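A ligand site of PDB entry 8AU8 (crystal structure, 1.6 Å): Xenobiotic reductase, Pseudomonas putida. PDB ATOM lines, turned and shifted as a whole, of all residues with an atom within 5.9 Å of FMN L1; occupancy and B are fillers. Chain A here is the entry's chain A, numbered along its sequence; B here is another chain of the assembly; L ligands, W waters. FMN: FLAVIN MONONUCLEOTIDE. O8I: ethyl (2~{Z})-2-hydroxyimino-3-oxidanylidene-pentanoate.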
ATOM      1  N   PRO A  22     -31.171 -11.459  16.729  1.00  0.00           N
ATOM      2  CA  PRO A  22     -31.036 -10.011  16.703  1.00  0.00           C
ATOM      3  C   PRO A  22     -31.265  -9.489  15.305  1.00  0.00           C
ATOM      4  O   PRO A  22     -31.218 -10.255  14.331  1.00  0.00           O
ATOM      5  CB  PRO A  22     -29.586  -9.796  17.153  1.00  0.00           C
ATOM      6  CG  PRO A  22     -28.866 -11.014  16.548  1.00  0.00           C
ATOM      7  CD  PRO A  22     -29.867 -12.150  16.644  1.00  0.00           C
ATOM      8  N   PRO A  23     -31.497  -8.179  15.152  1.00  0.00           N
ATOM      9  CA  PRO A  23     -31.708  -7.617  13.812  1.00  0.00           C
ATOM     10  C   PRO A  23     -30.496  -7.843  12.925  1.00  0.00           C
ATOM     11  O   PRO A  23     -29.351  -7.575  13.323  1.00  0.00           O
ATOM     12  CB  PRO A  23     -31.954  -6.129  14.087  1.00  0.00           C
ATOM     13  CG  PRO A  23     -31.303  -5.887  15.445  1.00  0.00           C
ATOM     14  CD  PRO A  23     -31.510  -7.157  16.211  1.00  0.00           C
ATOM     15  N   MET A  24     -30.736  -8.353  11.699  1.00  0.00           N
ATOM     16  CA  MET A  24     -29.673  -8.575  10.731  1.00  0.00           C
ATOM     17  C   MET A  24     -30.132  -8.115   9.348  1.00  0.00           C
ATOM     18  O   MET A  24     -30.899  -8.826   8.694  1.00  0.00           O
ATOM     19  CB  MET A  24     -29.229 -10.036  10.714  1.00  0.00           C
ATOM     20  CG  MET A  24     -28.362 -10.395  11.908  1.00  0.00           C
ATOM     21  SD  MET A  24     -27.933 -12.150  11.844  1.00  0.00           S
ATOM     22  CE  MET A  24     -29.549 -12.920  12.045  1.00  0.00           C
ATOM     23  N   CYS A  25     -29.658  -6.940   8.930  1.00  0.00           N
ATOM     24  CA  CYS A  25     -29.881  -6.414   7.597  1.00  0.00           C
ATOM     25  C   CYS A  25     -29.591  -7.457   6.532  1.00  0.00           C
ATOM     26  O   CYS A  25     -28.547  -8.125   6.564  1.00  0.00           O
ATOM     27  CB  CYS A  25     -28.988  -5.200   7.359  1.00  0.00           C
ATOM     28  SG  CYS A  25     -29.616  -3.683   8.087  1.00  0.00           S
ATOM     29  N   GLN A  26     -30.499  -7.552   5.561  1.00  0.00           N
ATOM     30  CA  GLN A  26     -30.388  -8.473   4.440  1.00  0.00           C
ATOM     31  C   GLN A  26     -29.997  -7.793   3.138  1.00  0.00           C
ATOM     32  O   GLN A  26     -29.545  -8.472   2.214  1.00  0.00           O
ATOM     33  CB  GLN A  26     -31.727  -9.204   4.240  1.00  0.00           C
ATOM     34  CG  GLN A  26     -32.105 -10.088   5.433  1.00  0.00           C
ATOM     35  CD  GLN A  26     -31.068 -11.167   5.714  1.00  0.00           C
ATOM     36  OE1 GLN A  26     -30.991 -12.155   4.998  1.00  0.00           O
ATOM     37  NE2 GLN A  26     -30.263 -10.985   6.759  1.00  0.00           N
ATOM     38  N   TYR A  27     -30.175  -6.464   3.048  1.00  0.00           N
ATOM     39  CA  TYR A  27     -29.799  -5.671   1.874  1.00  0.00           C
ATOM     40  C   TYR A  27     -30.476  -6.194   0.597  1.00  0.00           C
ATOM     41  O   TYR A  27     -29.924  -6.111  -0.492  1.00  0.00           O
ATOM     42  CB  TYR A  27     -28.274  -5.620   1.710  1.00  0.00           C
ATOM     43  CG  TYR A  27     -27.529  -5.246   2.977  1.00  0.00           C
ATOM     44  CD1 TYR A  27     -27.349  -3.915   3.344  1.00  0.00           C
ATOM     45  CD2 TYR A  27     -27.022  -6.232   3.836  1.00  0.00           C
ATOM     46  CE1 TYR A  27     -26.674  -3.572   4.518  1.00  0.00           C
ATOM     47  CE2 TYR A  27     -26.340  -5.894   5.014  1.00  0.00           C
ATOM     48  CZ  TYR A  27     -26.171  -4.558   5.336  1.00  0.00           C
ATOM     49  OH  TYR A  27     -25.512  -4.213   6.494  1.00  0.00           O
ATOM     50  N   GLU A  56     -34.646  -6.985  10.988  1.00  0.00           N
ATOM     51  CA  GLU A  56     -33.543  -6.100  10.643  1.00  0.00           C
ATOM     52  C   GLU A  56     -33.875  -4.614  10.743  1.00  0.00           C
ATOM     53  O   GLU A  56     -35.042  -4.224  10.625  1.00  0.00           O
ATOM     54  CB  GLU A  56     -33.077  -6.396   9.215  1.00  0.00           C
ATOM     55  CG  GLU A  56     -34.143  -6.029   8.177  1.00  0.00           C
ATOM     56  CD  GLU A  56     -33.850  -6.662   6.821  1.00  0.00           C
ATOM     57  OE1 GLU A  56     -33.102  -6.042   6.024  1.00  0.00           O
ATOM     58  OE2 GLU A  56     -34.362  -7.783   6.558  1.00  0.00           O
ATOM     59  N   ALA A  57     -32.833  -3.796  10.915  1.00  0.00           N
ATOM     60  CA  ALA A  57     -32.917  -2.334  10.900  1.00  0.00           C
ATOM     61  C   ALA A  57     -33.771  -1.858   9.744  1.00  0.00           C
ATOM     62  O   ALA A  57     -33.435  -2.067   8.574  1.00  0.00           O
ATOM     63  CB  ALA A  57     -31.530  -1.733  10.777  1.00  0.00           C
ATOM     64  N   GLN A  99     -36.646  -3.711  14.599  1.00  0.00           N
ATOM     65  CA  GLN A  99     -35.730  -2.625  14.919  1.00  0.00           C
ATOM     66  C   GLN A  99     -35.962  -1.481  13.935  1.00  0.00           C
ATOM     67  O   GLN A  99     -35.814  -1.671  12.726  1.00  0.00           O
ATOM     68  CB  GLN A  99     -34.278  -3.103  14.830  1.00  0.00           C
ATOM     69  CG  GLN A  99     -33.287  -2.052  15.350  1.00  0.00           C
ATOM     70  CD  GLN A  99     -31.854  -2.390  15.011  1.00  0.00           C
ATOM     71  OE1 GLN A  99     -31.506  -2.533  13.846  1.00  0.00           O
ATOM     72  NE2 GLN A  99     -31.010  -2.504  16.051  1.00  0.00           N
ATOM     73  N   GLU A 176     -37.632  -2.242  18.908  1.00  0.00           N
ATOM     74  CA  GLU A 176     -36.269  -1.909  19.317  1.00  0.00           C
ATOM     75  C   GLU A 176     -35.845  -0.633  18.591  1.00  0.00           C
ATOM     76  O   GLU A 176     -35.800  -0.609  17.360  1.00  0.00           O
ATOM     77  CB  GLU A 176     -35.300  -3.043  19.011  1.00  0.00           C
ATOM     78  CG  GLU A 176     -33.881  -2.796  19.528  1.00  0.00           C
ATOM     79  CD  GLU A 176     -32.930  -3.914  19.109  1.00  0.00           C
ATOM     80  OE1 GLU A 176     -33.087  -5.055  19.605  1.00  0.00           O
ATOM     81  OE2 GLU A 176     -32.045  -3.657  18.268  1.00  0.00           O
ATOM     82  N   HIS A 178     -33.094   1.789  17.333  1.00  0.00           N
ATOM     83  CA  HIS A 178     -31.686   1.538  16.995  1.00  0.00           C
ATOM     84  C   HIS A 178     -30.839   2.743  17.385  1.00  0.00           C
ATOM     85  O   HIS A 178     -30.585   3.636  16.581  1.00  0.00           O
ATOM     86  CB  HIS A 178     -31.506   1.220  15.519  1.00  0.00           C
ATOM     87  CG  HIS A 178     -30.181   0.619  15.219  1.00  0.00           C
ATOM     88  ND1 HIS A 178     -29.176   0.527  16.159  1.00  0.00           N
ATOM     89  CD2 HIS A 178     -29.691   0.017  14.104  1.00  0.00           C
ATOM     90  CE1 HIS A 178     -28.125  -0.071  15.631  1.00  0.00           C
ATOM     91  NE2 HIS A 178     -28.409  -0.400  14.384  1.00  0.00           N
ATOM     92  N   ALA A 180     -27.641   2.443  18.384  1.00  0.00           N
ATOM     93  CA  ALA A 180     -26.294   1.879  18.524  1.00  0.00           C
ATOM     94  C   ALA A 180     -25.527   1.955  17.208  1.00  0.00           C
ATOM     95  O   ALA A 180     -26.028   2.454  16.195  1.00  0.00           O
ATOM     96  CB  ALA A 180     -26.383   0.431  19.023  1.00  0.00           C
ATOM     97  N   HIS A 181     -24.279   1.491  17.240  1.00  0.00           N
ATOM     98  CA  HIS A 181     -23.499   1.161  16.055  1.00  0.00           C
ATOM     99  C   HIS A 181     -23.170   2.363  15.183  1.00  0.00           C
ATOM    100  O   HIS A 181     -22.918   2.213  13.972  1.00  0.00           O
ATOM    101  CB  HIS A 181     -24.207   0.056  15.252  1.00  0.00           C
ATOM    102  CG  HIS A 181     -24.407  -1.219  16.022  1.00  0.00           C
ATOM    103  ND1 HIS A 181     -25.166  -2.268  15.559  1.00  0.00           N
ATOM    104  CD2 HIS A 181     -23.929  -1.601  17.229  1.00  0.00           C
ATOM    105  CE1 HIS A 181     -25.161  -3.243  16.459  1.00  0.00           C
ATOM    106  NE2 HIS A 181     -24.409  -2.864  17.467  1.00  0.00           N
ATOM    107  N   ARG A 231     -31.476  -0.635  21.318  1.00  0.00           N
ATOM    108  CA  ARG A 231     -30.088  -1.066  21.255  1.00  0.00           C
ATOM    109  C   ARG A 231     -29.206   0.161  21.398  1.00  0.00           C
ATOM    110  O   ARG A 231     -29.472   1.220  20.819  1.00  0.00           O
ATOM    111  CB  ARG A 231     -29.796  -1.782  19.926  1.00  0.00           C
ATOM    112  CG  ARG A 231     -28.525  -2.618  19.971  1.00  0.00           C
ATOM    113  CD  ARG A 231     -28.464  -3.612  18.812  1.00  0.00           C
ATOM    114  NE  ARG A 231     -27.611  -4.746  19.171  1.00  0.00           N
ATOM    115  CZ  ARG A 231     -27.329  -5.752  18.350  1.00  0.00           C
ATOM    116  NH1 ARG A 231     -27.706  -5.743  17.083  1.00  0.00           N
ATOM    117  NH2 ARG A 231     -26.634  -6.790  18.817  1.00  0.00           N
ATOM    118  N   SER A 266     -24.589  -3.052  23.282  1.00  0.00           N
ATOM    119  CA  SER A 266     -23.681  -3.273  22.152  1.00  0.00           C
ATOM    120  C   SER A 266     -22.492  -2.320  22.283  1.00  0.00           C
ATOM    121  O   SER A 266     -22.257  -1.709  23.327  1.00  0.00           O
ATOM    122  CB  SER A 266     -24.431  -3.107  20.819  1.00  0.00           C
ATOM    123  OG  SER A 266     -23.699  -3.755  19.780  1.00  0.00           O
ATOM    124  N   ALA A 301     -24.832  -9.662  22.167  1.00  0.00           N
ATOM    125  CA  ALA A 301     -24.490 -10.521  21.031  1.00  0.00           C
ATOM    126  C   ALA A 301     -22.981 -10.443  20.856  1.00  0.00           C
ATOM    127  O   ALA A 301     -22.268 -10.005  21.766  1.00  0.00           O
ATOM    128  CB  ALA A 301     -25.253 -10.064  19.763  1.00  0.00           C
ATOM    129  N   TRP A 302     -22.504 -10.851  19.678  1.00  0.00           N
ATOM    130  CA  TRP A 302     -21.102 -10.723  19.262  1.00  0.00           C
ATOM    131  C   TRP A 302     -20.277 -11.835  19.880  1.00  0.00           C
ATOM    132  O   TRP A 302     -19.329 -11.580  20.636  1.00  0.00           O
ATOM    133  CB  TRP A 302     -20.500  -9.344  19.605  1.00  0.00           C
ATOM    134  CG  TRP A 302     -21.290  -8.128  19.108  1.00  0.00           C
ATOM    135  CD1 TRP A 302     -22.097  -7.296  19.857  1.00  0.00           C
ATOM    136  CD2 TRP A 302     -21.330  -7.612  17.762  1.00  0.00           C
ATOM    137  NE1 TRP A 302     -22.627  -6.297  19.056  1.00  0.00           N
ATOM    138  CE2 TRP A 302     -22.181  -6.478  17.769  1.00  0.00           C
ATOM    139  CE3 TRP A 302     -20.735  -8.001  16.560  1.00  0.00           C
ATOM    140  CZ2 TRP A 302     -22.441  -5.744  16.612  1.00  0.00           C
ATOM    141  CZ3 TRP A 302     -20.992  -7.269  15.420  1.00  0.00           C
ATOM    142  CH2 TRP A 302     -21.841  -6.141  15.460  1.00  0.00           C
ATOM    143  N   GLY A 303     -20.632 -13.071  19.581  1.00  0.00           N
ATOM    144  CA  GLY A 303     -19.872 -14.219  19.999  1.00  0.00           C
ATOM    145  C   GLY A 303     -20.495 -15.113  21.060  1.00  0.00           C
ATOM    146  O   GLY A 303     -19.751 -15.847  21.731  1.00  0.00           O
ATOM    147  N   PHE A 304     -21.816 -15.054  21.260  1.00  0.00           N
ATOM    148  CA  PHE A 304     -22.494 -16.008  22.144  1.00  0.00           C
ATOM    149  C   PHE A 304     -23.046 -17.205  21.381  1.00  0.00           C
ATOM    150  O   PHE A 304     -23.738 -18.033  21.989  1.00  0.00           O
ATOM    151  CB  PHE A 304     -23.633 -15.329  22.919  1.00  0.00           C
ATOM    152  CG  PHE A 304     -23.195 -14.259  23.881  1.00  0.00           C
ATOM    153  CD1 PHE A 304     -22.811 -14.577  25.184  1.00  0.00           C
ATOM    154  CD2 PHE A 304     -23.214 -12.929  23.488  1.00  0.00           C
ATOM    155  CE1 PHE A 304     -22.433 -13.586  26.073  1.00  0.00           C
ATOM    156  CE2 PHE A 304     -22.823 -11.920  24.373  1.00  0.00           C
ATOM    157  CZ  PHE A 304     -22.432 -12.250  25.673  1.00  0.00           C
ATOM    158  N   GLY A 305     -22.744 -17.323  20.095  1.00  0.00           N
ATOM    159  CA  GLY A 305     -23.369 -18.311  19.230  1.00  0.00           C
ATOM    160  C   GLY A 305     -22.855 -19.742  19.306  1.00  0.00           C
ATOM    161  O   GLY A 305     -22.773 -20.415  18.281  1.00  0.00           O
ATOM    162  N   SER A 323     -28.711 -13.155  22.272  1.00  0.00           N
ATOM    163  CA  SER A 323     -28.905 -12.876  20.844  1.00  0.00           C
ATOM    164  C   SER A 323     -27.872 -13.647  20.038  1.00  0.00           C
ATOM    165  O   SER A 323     -26.662 -13.534  20.291  1.00  0.00           O
ATOM    166  CB  SER A 323     -28.807 -11.375  20.572  1.00  0.00           C
ATOM    167  OG  SER A 323     -29.870 -10.715  21.236  1.00  0.00           O
ATOM    168  N   VAL A 324     -28.350 -14.434  19.067  1.00  0.00           N
ATOM    169  CA  VAL A 324     -27.517 -15.332  18.268  1.00  0.00           C
ATOM    170  C   VAL A 324     -27.807 -15.004  16.811  1.00  0.00           C
ATOM    171  O   VAL A 324     -28.874 -15.356  16.295  1.00  0.00           O
ATOM    172  CB  VAL A 324     -27.782 -16.804  18.590  1.00  0.00           C
ATOM    173  CG1 VAL A 324     -26.947 -17.757  17.705  1.00  0.00           C
ATOM    174  CG2 VAL A 324     -27.518 -17.067  20.097  1.00  0.00           C
ATOM    175  N   GLY A 325     -26.871 -14.321  16.167  1.00  0.00           N
ATOM    176  CA  GLY A 325     -27.067 -13.800  14.824  1.00  0.00           C
ATOM    177  C   GLY A 325     -26.530 -14.690  13.724  1.00  0.00           C
ATOM    178  O   GLY A 325     -27.285 -15.443  13.096  1.00  0.00           O
ATOM    179  N   ARG A 326     -25.225 -14.628  13.475  1.00  0.00           N
ATOM    180  CA  ARG A 326     -24.651 -15.311  12.310  1.00  0.00           C
ATOM    181  C   ARG A 326     -24.890 -16.816  12.340  1.00  0.00           C
ATOM    182  O   ARG A 326     -25.034 -17.442  11.279  1.00  0.00           O
ATOM    183  CB  ARG A 326     -23.166 -14.993  12.209  1.00  0.00           C
ATOM    184  CG  ARG A 326     -22.890 -13.607  11.635  1.00  0.00           C
ATOM    185  CD  ARG A 326     -21.439 -13.190  11.844  1.00  0.00           C
ATOM    186  NE  ARG A 326     -21.175 -12.919  13.248  1.00  0.00           N
ATOM    187  CZ  ARG A 326     -20.000 -12.533  13.725  1.00  0.00           C
ATOM    188  NH1 ARG A 326     -18.960 -12.325  12.926  1.00  0.00           N
ATOM    189  NH2 ARG A 326     -19.854 -12.347  15.036  1.00  0.00           N
ATOM    190  N   ALA A 327     -24.938 -17.426  13.530  1.00  0.00           N
ATOM    191  CA  ALA A 327     -25.193 -18.860  13.575  1.00  0.00           C
ATOM    192  C   ALA A 327     -26.558 -19.193  12.984  1.00  0.00           C
ATOM    193  O   ALA A 327     -26.755 -20.321  12.502  1.00  0.00           O
ATOM    194  CB  ALA A 327     -25.102 -19.376  15.016  1.00  0.00           C
ATOM    195  N   LEU A 329     -27.849 -17.464  10.381  1.00  0.00           N
ATOM    196  CA  LEU A 329     -27.652 -17.414   8.935  1.00  0.00           C
ATOM    197  C   LEU A 329     -27.070 -18.716   8.433  1.00  0.00           C
ATOM    198  O   LEU A 329     -27.474 -19.232   7.375  1.00  0.00           O
ATOM    199  CB  LEU A 329     -26.740 -16.243   8.570  1.00  0.00           C
ATOM    200  CG  LEU A 329     -27.118 -14.845   9.095  1.00  0.00           C
ATOM    201  CD1 LEU A 329     -26.144 -13.836   8.536  1.00  0.00           C
ATOM    202  CD2 LEU A 329     -28.556 -14.464   8.705  1.00  0.00           C
ATOM    203  N   PRO B 354     -26.510 -12.646   0.979  1.00  0.00           N
ATOM    204  CA  PRO B 354     -26.831 -12.083   2.307  1.00  0.00           C
ATOM    205  C   PRO B 354     -26.431 -12.968   3.465  1.00  0.00           C
ATOM    206  O   PRO B 354     -26.423 -12.499   4.616  1.00  0.00           O
ATOM    207  CB  PRO B 354     -28.361 -11.910   2.265  1.00  0.00           C
ATOM    208  CG  PRO B 354     -28.692 -11.843   0.799  1.00  0.00           C
ATOM    209  CD  PRO B 354     -27.718 -12.788   0.138  1.00  0.00           C
ATOM    210  N   TRP B 358     -21.057 -12.941   5.162  1.00  0.00           N
ATOM    211  CA  TRP B 358     -20.763 -12.860   6.582  1.00  0.00           C
ATOM    212  C   TRP B 358     -20.144 -14.134   7.131  1.00  0.00           C
ATOM    213  O   TRP B 358     -19.370 -14.085   8.083  1.00  0.00           O
ATOM    214  CB  TRP B 358     -22.053 -12.535   7.347  1.00  0.00           C
ATOM    215  CG  TRP B 358     -22.733 -11.377   6.706  1.00  0.00           C
ATOM    216  CD1 TRP B 358     -23.849 -11.413   5.911  1.00  0.00           C
ATOM    217  CD2 TRP B 358     -22.305 -10.016   6.738  1.00  0.00           C
ATOM    218  NE1 TRP B 358     -24.146 -10.152   5.472  1.00  0.00           N
ATOM    219  CE2 TRP B 358     -23.216  -9.273   5.954  1.00  0.00           C
ATOM    220  CE3 TRP B 358     -21.236  -9.351   7.340  1.00  0.00           C
ATOM    221  CZ2 TRP B 358     -23.097  -7.895   5.788  1.00  0.00           C
ATOM    222  CZ3 TRP B 358     -21.124  -7.985   7.171  1.00  0.00           C
ATOM    223  CH2 TRP B 358     -22.046  -7.270   6.401  1.00  0.00           C
ATOM    224  N   ARG B 361     -16.212 -14.567   6.572  1.00  0.00           N
ATOM    225  CA  ARG B 361     -15.348 -13.886   7.531  1.00  0.00           C
ATOM    226  C   ARG B 361     -15.638 -14.299   8.973  1.00  0.00           C
ATOM    227  O   ARG B 361     -16.361 -15.266   9.228  1.00  0.00           O
ATOM    228  CB  ARG B 361     -15.496 -12.379   7.377  1.00  0.00           C
ATOM    229  CG  ARG B 361     -16.272 -11.708   8.494  1.00  0.00           C
ATOM    230  CD  ARG B 361     -17.168 -10.592   7.959  1.00  0.00           C
ATOM    231  NE  ARG B 361     -17.742  -9.774   9.020  1.00  0.00           N
ATOM    232  CZ  ARG B 361     -18.632 -10.206   9.906  1.00  0.00           C
ATOM    233  NH1 ARG B 361     -19.030 -11.476   9.923  1.00  0.00           N
ATOM    234  NH2 ARG B 361     -19.129  -9.359  10.794  1.00  0.00           N
HETATM  235  N1  FMN L   1     -27.212  -5.022  14.236  1.00  0.00           N
HETATM  236  C2  FMN L   1     -28.289  -4.164  14.384  1.00  0.00           C
HETATM  237  O2  FMN L   1     -28.449  -3.568  15.461  1.00  0.00           O
HETATM  238  N3  FMN L   1     -29.173  -3.977  13.331  1.00  0.00           N
HETATM  239  C4  FMN L   1     -29.001  -4.628  12.125  1.00  0.00           C
HETATM  240  O4  FMN L   1     -29.822  -4.476  11.202  1.00  0.00           O
HETATM  241  C4A FMN L   1     -27.902  -5.473  11.978  1.00  0.00           C
HETATM  242  N5  FMN L   1     -27.699  -6.136  10.796  1.00  0.00           N
HETATM  243  C5A FMN L   1     -26.725  -7.093  10.722  1.00  0.00           C
HETATM  244  C6  FMN L   1     -26.658  -7.863   9.569  1.00  0.00           C
HETATM  245  C7  FMN L   1     -25.735  -8.883   9.447  1.00  0.00           C
HETATM  246  C7M FMN L   1     -25.725  -9.697   8.184  1.00  0.00           C
HETATM  247  C8  FMN L   1     -24.863  -9.122  10.509  1.00  0.00           C
HETATM  248  C8M FMN L   1     -23.850 -10.227  10.410  1.00  0.00           C
HETATM  249  C9  FMN L   1     -24.930  -8.344  11.669  1.00  0.00           C
HETATM  250  C9A FMN L   1     -25.868  -7.315  11.782  1.00  0.00           C
HETATM  251  N10 FMN L   1     -25.950  -6.545  12.937  1.00  0.00           N
HETATM  252  C10 FMN L   1     -27.016  -5.680  13.050  1.00  0.00           C
HETATM  253  C1' FMN L   1     -25.346  -7.064  14.232  1.00  0.00           C
HETATM  254  C2' FMN L   1     -26.033  -8.328  14.789  1.00  0.00           C
HETATM  255  O2' FMN L   1     -27.301  -8.006  15.304  1.00  0.00           O
HETATM  256  C3' FMN L   1     -25.233  -8.995  15.897  1.00  0.00           C
HETATM  257  O3' FMN L   1     -24.940  -8.074  16.927  1.00  0.00           O
HETATM  258  C4' FMN L   1     -23.929  -9.584  15.348  1.00  0.00           C
HETATM  259  O4' FMN L   1     -24.214 -10.447  14.274  1.00  0.00           O
HETATM  260  C5' FMN L   1     -23.130 -10.321  16.426  1.00  0.00           C
HETATM  261  O5' FMN L   1     -23.792 -11.466  16.908  1.00  0.00           O
HETATM  262  P   FMN L   1     -23.326 -12.929  16.387  1.00  0.00           P
HETATM  263  O1P FMN L   1     -24.250 -13.921  17.039  1.00  0.00           O
HETATM  264  O2P FMN L   1     -23.423 -12.938  14.886  1.00  0.00           O
HETATM  265  O3P FMN L   1     -21.895 -13.160  16.840  1.00  0.00           O
HETATM  266  N1  O8I L   2     -24.711  -3.933  10.331  1.00  0.00           N
HETATM  267  C4  O8I L   2     -23.853  -3.494  12.719  1.00  0.00           C
HETATM  268  C5  O8I L   2     -28.181  -1.330  11.178  1.00  0.00           C
HETATM  269  C6  O8I L   2     -21.847  -2.742  13.681  1.00  0.00           C
HETATM  270  C7  O8I L   2     -20.636  -1.995  13.130  1.00  0.00           C
HETATM  271  C1  O8I L   2     -27.074  -2.272  10.747  1.00  0.00           C
HETATM  272  C2  O8I L   2     -26.155  -2.560  11.925  1.00  0.00           C
HETATM  273  C3  O8I L   2     -24.907  -3.356  11.638  1.00  0.00           C
HETATM  274  O1  O8I L   2     -22.936  -2.448  12.855  1.00  0.00           O
HETATM  275  O2  O8I L   2     -26.412  -2.172  13.014  1.00  0.00           O
HETATM  276  O3  O8I L   2     -23.807  -4.450  13.430  1.00  0.00           O
HETATM  277  O4  O8I L   2     -23.479  -4.610  10.320  1.00  0.00           O
HETATM  278  O   HOH W   1     -23.972 -13.858  19.711  1.00  0.00           O
HETATM  279  O   HOH W   2     -21.419 -15.751  17.804  1.00  0.00           O
HETATM  280  O   HOH W   3     -24.004 -16.467  16.035  1.00  0.00           O
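The backbone NH of Arg 326 sits at hydrogen-bond distance from an oxygen (O2P) of FMN L1, 2.8 Å away. O2P of FMN L1 is in salt-bridge range of NE of Arg 326 (2.8 Å). The backbone NH (N) of Gly 325 lies within hydrogen-bond range of an oxygen (O1P) of FMN L1, 2.8 Å away. A nitrogen (N3) of FMN L1 is in hydrogen-bond range of the side-chain amide oxygen of Gln 99. The guanidinium group of Arg 231 sits at hydrogen-bond distance from an oxygen (O2) of FMN L1, 2.8 Å away. The backbone NH (N) of Cys 25 sits at hydrogen-bond distance from a nitrogen (N5) of FMN L1 (2.8 Å). The side-chain sulfur of Cys 25 lies within hydrogen-bond range of an oxygen (O4) of FMN L1 (3.2 Å). O2' of FMN L1 sits at hydrogen-bond distance from O of Pro 23. An oxygen (O3P) of FMN L1 is in hydrogen-bond range of the backbone NH (N) of Gly 303 (3.0 Å). An oxygen (O4) of FMN L1 sits at hydrogen-bond distance from the backbone NH of Ala 57, at 3.1 Å. N of Trp 302 sits at hydrogen-bond distance from O5' of FMN L1. NE2 of His 178 sits at hydrogen-bond distance from O2 of FMN L1. A ring nitrogen (NE2) of His 178 sits at hydrogen-bond distance from an oxygen (O2) of O8I L2 (3.0 Å). O2 of O8I L2 is in hydrogen-bond range of ND1 of His 181 (2.8 Å).
O2 of O8I L2 sits close to N3 of FMN L1 (3.3 Å).
The side-chain amide oxygen (OE1) of Gln 99 sits close to the backbone NH (N) of Ala 57 (3.5 Å). OE2 of Glu 176 sits at hydrogen-bond distance from NE2 of Gln 99 (2.7 Å). The backbone NH of Ala 180 sits at hydrogen-bond distance from the backbone carbonyl oxygen of Arg 231 (3.3 Å). The side-chain hydroxyl (OG) of Ser 266 lies within hydrogen-bond range of the indole nitrogen (NE1) of Trp 302 (2.9 Å). O of Met 24 lies within hydrogen-bond range of NE2 of Gln 26. The backbone carbonyl oxygen (O) of Trp 358 of chain B sits at hydrogen-bond distance from the guanidinium group (NH1) of Arg 361 of chain B (3.2 Å). The backbone NH (N) of Ala 180 is in hydrogen-bond range of a ring nitrogen (ND1) of His 178. The side-chain hydroxyl of Ser 266 sits at hydrogen-bond distance from a ring nitrogen (NE2) of His 181 (2.6 Å).
Residues that only touch FMN L1: Pro 22 (3.4 Å), Met 24 (3.1 Å), His 181 (3.5 Å), Ala 301 (3.5 Å), Val 324 (3.7 Å) and Trp 358 of chain B (3.2 Å). 16 residues have an atom within 4 Å of FMN L1: Pro 22, Pro 23, Met 24, Cys 25, Ala 57, Gln 99, His 178, His 181, Arg 231, Ala 301, Trp 302, Gly 303, Val 324, Gly 325, Arg 326 and Trp 358 of chain B. Along chain A the residues within 4 Å of FMN L1 span positions 22 to 326.
Water W3 lies within hydrogen-bond range of O1P of FMN L1 (2.7 Å), N of Ala 327 (2.8 Å) and N of Arg 326 (3.4 Å). Water W2 lies within hydrogen-bond range of an oxygen (O3P) of FMN L1 (2.8 Å), the backbone NH of Gly 305 (3.1 Å) and the backbone NH of Gly 303 (3.3 Å).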
